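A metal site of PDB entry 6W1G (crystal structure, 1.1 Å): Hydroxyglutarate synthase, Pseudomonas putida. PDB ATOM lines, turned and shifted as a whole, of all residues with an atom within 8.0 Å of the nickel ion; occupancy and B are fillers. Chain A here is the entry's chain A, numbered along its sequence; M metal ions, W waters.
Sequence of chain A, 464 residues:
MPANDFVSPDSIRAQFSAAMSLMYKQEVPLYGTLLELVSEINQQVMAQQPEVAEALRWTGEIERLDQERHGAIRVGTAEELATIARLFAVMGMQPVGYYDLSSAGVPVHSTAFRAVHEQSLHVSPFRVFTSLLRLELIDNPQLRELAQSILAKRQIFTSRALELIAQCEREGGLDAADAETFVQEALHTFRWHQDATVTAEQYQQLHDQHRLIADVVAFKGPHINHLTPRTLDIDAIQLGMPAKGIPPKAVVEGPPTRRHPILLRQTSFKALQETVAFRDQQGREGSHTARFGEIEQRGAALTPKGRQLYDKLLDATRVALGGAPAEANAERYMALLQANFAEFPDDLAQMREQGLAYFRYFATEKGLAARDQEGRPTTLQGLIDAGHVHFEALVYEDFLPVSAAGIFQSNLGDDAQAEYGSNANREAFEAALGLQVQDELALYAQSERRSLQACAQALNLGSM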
ATOM      1  N   HIS A  70      16.953  17.268  14.611  1.00  0.00           N
ATOM      2  CA  HIS A  70      18.384  17.075  14.765  1.00  0.00           C
ATOM      3  C   HIS A  70      18.791  17.454  16.188  1.00  0.00           C
ATOM      4  O   HIS A  70      18.182  18.331  16.791  1.00  0.00           O
ATOM      5  CB  HIS A  70      19.309  17.786  13.753  1.00  0.00           C
ATOM      6  CG  HIS A  70      19.545  19.252  13.936  1.00  0.00           C
ATOM      7  ND1 HIS A  70      18.875  20.219  13.223  1.00  0.00           N
ATOM      8  CD2 HIS A  70      20.448  19.909  14.708  1.00  0.00           C
ATOM      9  CE1 HIS A  70      19.333  21.412  13.571  1.00  0.00           C
ATOM     10  NE2 HIS A  70      20.281  21.260  14.482  1.00  0.00           N
ATOM     11  N   GLY A  71      19.808  16.804  16.714  1.00  0.00           N
ATOM     12  CA  GLY A  71      20.454  17.244  17.929  1.00  0.00           C
ATOM     13  C   GLY A  71      21.816  17.813  17.615  1.00  0.00           C
ATOM     14  O   GLY A  71      22.368  17.593  16.537  1.00  0.00           O
ATOM     15  N   ALA A  72      22.362  18.555  18.580  1.00  0.00           N
ATOM     16  CA  ALA A  72      23.712  19.077  18.494  1.00  0.00           C
ATOM     17  C   ALA A  72      24.384  18.859  19.837  1.00  0.00           C
ATOM     18  O   ALA A  72      23.787  19.159  20.886  1.00  0.00           O
ATOM     19  CB  ALA A  72      23.676  20.577  18.182  1.00  0.00           C
ATOM     20  N   ILE A  73      25.611  18.348  19.802  1.00  0.00           N
ATOM     21  CA  ILE A  73      26.427  18.061  20.958  1.00  0.00           C
ATOM     22  C   ILE A  73      27.861  18.445  20.658  1.00  0.00           C
ATOM     23  O   ILE A  73      28.278  18.621  19.513  1.00  0.00           O
ATOM     24  CB  ILE A  73      26.386  16.558  21.311  1.00  0.00           C
ATOM     25  CG1 ILE A  73      26.927  15.675  20.174  1.00  0.00           C
ATOM     26  CG2 ILE A  73      24.997  16.190  21.722  1.00  0.00           C
ATOM     27  CD1 ILE A  73      27.119  14.206  20.498  1.00  0.00           C
ATOM     28  N   PHE A 129      24.521  16.637  14.972  1.00  0.00           N
ATOM     29  CA  PHE A 129      25.654  17.494  14.642  1.00  0.00           C
ATOM     30  C   PHE A 129      26.612  17.454  15.822  1.00  0.00           C
ATOM     31  O   PHE A 129      26.212  17.768  16.955  1.00  0.00           O
ATOM     32  CB  PHE A 129      25.151  18.920  14.421  1.00  0.00           C
ATOM     33  CG  PHE A 129      26.174  19.858  13.857  1.00  0.00           C
ATOM     34  CD1 PHE A 129      26.981  20.633  14.686  1.00  0.00           C
ATOM     35  CD2 PHE A 129      26.366  19.937  12.498  1.00  0.00           C
ATOM     36  CE1 PHE A 129      27.911  21.489  14.128  1.00  0.00           C
ATOM     37  CE2 PHE A 129      27.314  20.817  11.961  1.00  0.00           C
ATOM     38  CZ  PHE A 129      28.066  21.570  12.774  1.00  0.00           C
ATOM     39  N   ASN A 225      23.011  20.487  23.229  1.00  0.00           N
ATOM     40  CA  ASN A 225      23.154  21.916  22.975  1.00  0.00           C
ATOM     41  C   ASN A 225      21.884  22.506  22.392  1.00  0.00           C
ATOM     42  O   ASN A 225      21.503  23.650  22.704  1.00  0.00           O
ATOM     43  CB  ASN A 225      24.285  22.143  21.985  1.00  0.00           C
ATOM     44  CG  ASN A 225      24.555  23.584  21.722  1.00  0.00           C
ATOM     45  OD1 ASN A 225      24.304  24.052  20.613  1.00  0.00           O
ATOM     46  ND2 ASN A 225      25.064  24.309  22.703  1.00  0.00           N
ATOM     47  N   HIS A 226      21.235  21.745  21.538  1.00  0.00           N
ATOM     48  CA  HIS A 226      19.857  22.030  21.137  1.00  0.00           C
ATOM     49  C   HIS A 226      19.319  20.767  20.469  1.00  0.00           C
ATOM     50  O   HIS A 226      20.075  19.890  20.016  1.00  0.00           O
ATOM     51  CB  HIS A 226      19.723  23.270  20.254  1.00  0.00           C
ATOM     52  CG  HIS A 226      20.564  23.234  19.028  1.00  0.00           C
ATOM     53  ND1 HIS A 226      21.792  23.834  18.954  1.00  0.00           N
ATOM     54  CD2 HIS A 226      20.361  22.663  17.809  1.00  0.00           C
ATOM     55  CE1 HIS A 226      22.307  23.664  17.751  1.00  0.00           C
ATOM     56  NE2 HIS A 226      21.455  22.960  17.023  1.00  0.00           N
ATOM     57  N   LEU A 227      18.001  20.702  20.412  1.00  0.00           N
ATOM     58  CA  LEU A 227      17.255  19.709  19.668  1.00  0.00           C
ATOM     59  C   LEU A 227      16.255  20.481  18.808  1.00  0.00           C
ATOM     60  O   LEU A 227      15.417  21.201  19.366  1.00  0.00           O
ATOM     61  CB  LEU A 227      16.527  18.822  20.644  1.00  0.00           C
ATOM     62  CG  LEU A 227      16.120  17.492  20.275  1.00  0.00           C
ATOM     63  CD1 LEU A 227      16.904  16.626  19.488  1.00  0.00           C
ATOM     64  CD2 LEU A 227      15.354  16.780  21.290  1.00  0.00           C
ATOM     65  N   THR A 228      16.357  20.327  17.499  1.00  0.00           N
ATOM     66  CA  THR A 228      15.689  21.214  16.542  1.00  0.00           C
ATOM     67  C   THR A 228      14.639  20.433  15.771  1.00  0.00           C
ATOM     68  O   THR A 228      14.997  19.485  15.042  1.00  0.00           O
ATOM     69  CB  THR A 228      16.724  21.776  15.564  1.00  0.00           C
ATOM     70  OG1 THR A 228      17.697  22.456  16.344  1.00  0.00           O
ATOM     71  CG2 THR A 228      16.061  22.699  14.572  1.00  0.00           C
ATOM     72  N   GLU A 253      19.195  32.579   9.511  1.00  0.00           N
ATOM     73  CA  GLU A 253      20.314  32.066   8.733  1.00  0.00           C
ATOM     74  C   GLU A 253      19.800  31.242   7.581  1.00  0.00           C
ATOM     75  O   GLU A 253      18.763  30.584   7.702  1.00  0.00           O
ATOM     76  CB  GLU A 253      21.213  31.190   9.607  1.00  0.00           C
ATOM     77  CG  GLU A 253      21.838  31.950  10.780  1.00  0.00           C
ATOM     78  CD  GLU A 253      22.778  31.068  11.547  1.00  0.00           C
ATOM     79  OE1 GLU A 253      22.340  30.457  12.555  1.00  0.00           O
ATOM     80  OE2 GLU A 253      23.934  30.921  11.113  1.00  0.00           O
ATOM     81  N   LEU A 264      18.757  25.037   4.051  1.00  0.00           N
ATOM     82  CA  LEU A 264      17.830  25.148   5.169  1.00  0.00           C
ATOM     83  C   LEU A 264      17.825  26.606   5.624  1.00  0.00           C
ATOM     84  O   LEU A 264      18.732  27.371   5.296  1.00  0.00           O
ATOM     85  CB  LEU A 264      18.149  24.175   6.289  1.00  0.00           C
ATOM     86  CG  LEU A 264      19.448  24.387   7.046  1.00  0.00           C
ATOM     87  CD1 LEU A 264      19.356  25.476   8.093  1.00  0.00           C
ATOM     88  CD2 LEU A 264      19.843  23.088   7.730  1.00  0.00           C
ATOM     89  N   GLN A 266      17.256  28.712   9.459  1.00  0.00           N
ATOM     90  CA  GLN A 266      17.240  28.438  10.887  1.00  0.00           C
ATOM     91  C   GLN A 266      17.316  29.735  11.711  1.00  0.00           C
ATOM     92  O   GLN A 266      17.872  30.753  11.260  1.00  0.00           O
ATOM     93  CB  GLN A 266      18.396  27.544  11.325  1.00  0.00           C
ATOM     94  CG  GLN A 266      19.753  28.154  11.091  1.00  0.00           C
ATOM     95  CD  GLN A 266      20.964  27.238  11.328  1.00  0.00           C
ATOM     96  OE1 GLN A 266      20.952  26.018  11.049  1.00  0.00           O
ATOM     97  NE2 GLN A 266      22.033  27.846  11.831  1.00  0.00           N
ATOM     98  N   THR A 267      16.745  29.685  12.907  1.00  0.00           N
ATOM     99  CA  THR A 267      16.961  30.768  13.866  1.00  0.00           C
ATOM    100  C   THR A 267      16.926  30.155  15.262  1.00  0.00           C
ATOM    101  O   THR A 267      16.632  28.968  15.436  1.00  0.00           O
ATOM    102  CB  THR A 267      16.006  31.967  13.681  1.00  0.00           C
ATOM    103  OG1 THR A 267      16.452  33.044  14.495  1.00  0.00           O
ATOM    104  CG2 THR A 267      14.601  31.620  13.991  1.00  0.00           C
ATOM    105  N   GLY A 293      17.566  27.243  22.188  1.00  0.00           N
ATOM    106  CA  GLY A 293      16.852  26.398  21.257  1.00  0.00           C
ATOM    107  C   GLY A 293      17.011  26.901  19.840  1.00  0.00           C
ATOM    108  O   GLY A 293      17.602  27.945  19.540  1.00  0.00           O
ATOM    109  N   GLU A 294      16.517  26.076  18.916  1.00  0.00           N
ATOM    110  CA  GLU A 294      16.623  26.327  17.482  1.00  0.00           C
ATOM    111  C   GLU A 294      15.401  25.786  16.774  1.00  0.00           C
ATOM    112  O   GLU A 294      14.751  24.817  17.224  1.00  0.00           O
ATOM    113  CB  GLU A 294      17.903  25.668  16.968  1.00  0.00           C
ATOM    114  CG  GLU A 294      18.206  25.862  15.493  1.00  0.00           C
ATOM    115  CD  GLU A 294      19.529  25.243  15.155  1.00  0.00           C
ATOM    116  OE1 GLU A 294      19.615  24.017  14.986  1.00  0.00           O
ATOM    117  OE2 GLU A 294      20.534  25.993  15.092  1.00  0.00           O
ATOM    118  N   ILE A 295      15.102  26.385  15.633  1.00  0.00           N
ATOM    119  CA  ILE A 295      14.057  25.917  14.722  1.00  0.00           C
ATOM    120  C   ILE A 295      14.625  25.968  13.314  1.00  0.00           C
ATOM    121  O   ILE A 295      15.386  26.884  12.981  1.00  0.00           O
ATOM    122  CB  ILE A 295      12.777  26.811  14.865  1.00  0.00           C
ATOM    123  CG1 ILE A 295      11.649  26.362  13.996  1.00  0.00           C
ATOM    124  CG2 ILE A 295      13.070  28.292  14.624  1.00  0.00           C
ATOM    125  CD1 ILE A 295      11.143  24.994  14.276  1.00  0.00           C
ATOM    126  N   GLU A 296      14.227  25.016  12.464  1.00  0.00           N
ATOM    127  CA  GLU A 296      14.719  24.972  11.082  1.00  0.00           C
ATOM    128  C   GLU A 296      13.623  24.569  10.116  1.00  0.00           C
ATOM    129  O   GLU A 296      12.662  23.879  10.484  1.00  0.00           O
ATOM    130  CB  GLU A 296      15.910  24.026  10.918  1.00  0.00           C
ATOM    131  CG  GLU A 296      15.625  22.537  10.930  1.00  0.00           C
ATOM    132  CD  GLU A 296      16.902  21.645  10.987  1.00  0.00           C
ATOM    133  OE1 GLU A 296      17.984  22.170  10.785  1.00  0.00           O
ATOM    134  OE2 GLU A 296      16.832  20.441  11.257  1.00  0.00           O
ATOM    135  N   ARG A 298      13.713  22.878   6.152  1.00  0.00           N
ATOM    136  CA  ARG A 298      14.644  22.200   5.248  1.00  0.00           C
ATOM    137  C   ARG A 298      14.101  22.209   3.839  1.00  0.00           C
ATOM    138  O   ARG A 298      12.968  21.791   3.617  1.00  0.00           O
ATOM    139  CB  ARG A 298      14.952  20.768   5.715  1.00  0.00           C
ATOM    140  CG  ARG A 298      15.818  20.763   6.921  1.00  0.00           C
ATOM    141  CD  ARG A 298      16.140  19.344   7.426  1.00  0.00           C
ATOM    142  NE  ARG A 298      17.154  19.435   8.475  1.00  0.00           N
ATOM    143  CZ  ARG A 298      18.449  19.536   8.240  1.00  0.00           C
ATOM    144  NH1 ARG A 298      18.954  19.378   7.005  1.00  0.00           N
ATOM    145  NH2 ARG A 298      19.282  19.805   9.243  1.00  0.00           N
ATOM    146  N   PHE A 399      23.802  20.576   6.939  1.00  0.00           N
ATOM    147  CA  PHE A 399      23.778  21.834   7.685  1.00  0.00           C
ATOM    148  C   PHE A 399      24.378  22.947   6.836  1.00  0.00           C
ATOM    149  O   PHE A 399      24.998  22.687   5.785  1.00  0.00           O
ATOM    150  CB  PHE A 399      24.487  21.632   9.012  1.00  0.00           C
ATOM    151  CG  PHE A 399      23.753  20.622   9.862  1.00  0.00           C
ATOM    152  CD1 PHE A 399      22.733  21.039  10.660  1.00  0.00           C
ATOM    153  CD2 PHE A 399      23.997  19.269   9.781  1.00  0.00           C
ATOM    154  CE1 PHE A 399      21.981  20.164  11.387  1.00  0.00           C
ATOM    155  CE2 PHE A 399      23.212  18.370  10.471  1.00  0.00           C
ATOM    156  CZ  PHE A 399      22.254  18.806  11.322  1.00  0.00           C
HETATM  157 NI    NI M   1      21.398  22.966  14.973  1.00  0.00          NI
HETATM  158  O   HOH W   1      21.858  23.219  13.005  1.00  0.00           O
HETATM  159  O   HOH W   2      23.375  22.101  14.891  1.00  0.00           O
HETATM  160  O   HOH W   3      22.728  24.819  14.822  1.00  0.00           O
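The backbone carbonyl oxygen of His 226 lies within hydrogen-bond range of the backbone NH of Ala 72 (3.0 Å).
ND1 of His 226 is in hydrogen-bond range of OD1 of Asn 225 (3.0 Å).
The side-chain hydroxyl of Thr 228 lies close to the side-chain carboxylate of Glu 294 (2.8 Å).
N of Thr 228 is in hydrogen-bond range of O of His 70, at 2.8 Å.
The side-chain carboxylate (OE2) of Glu 296 lies within hydrogen-bond range of a ring nitrogen (ND1) of His 70, at 2.8 Å.
Residues that only touch the nickel ion: Thr 228.
Four residues have an atom within 4 Å of the nickel ion: His 70, His 226, Thr 228 and Glu 294.
The nearest printed residue that does not touch the nickel ion is Phe 399 (4.6 Å).
The nickel ion is bound by water W1, NE2 of His 226, OE1 of Glu 294, NE2 of His 70, water W2 and water W3.
The nickel ion has six donor atoms within binding distance.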
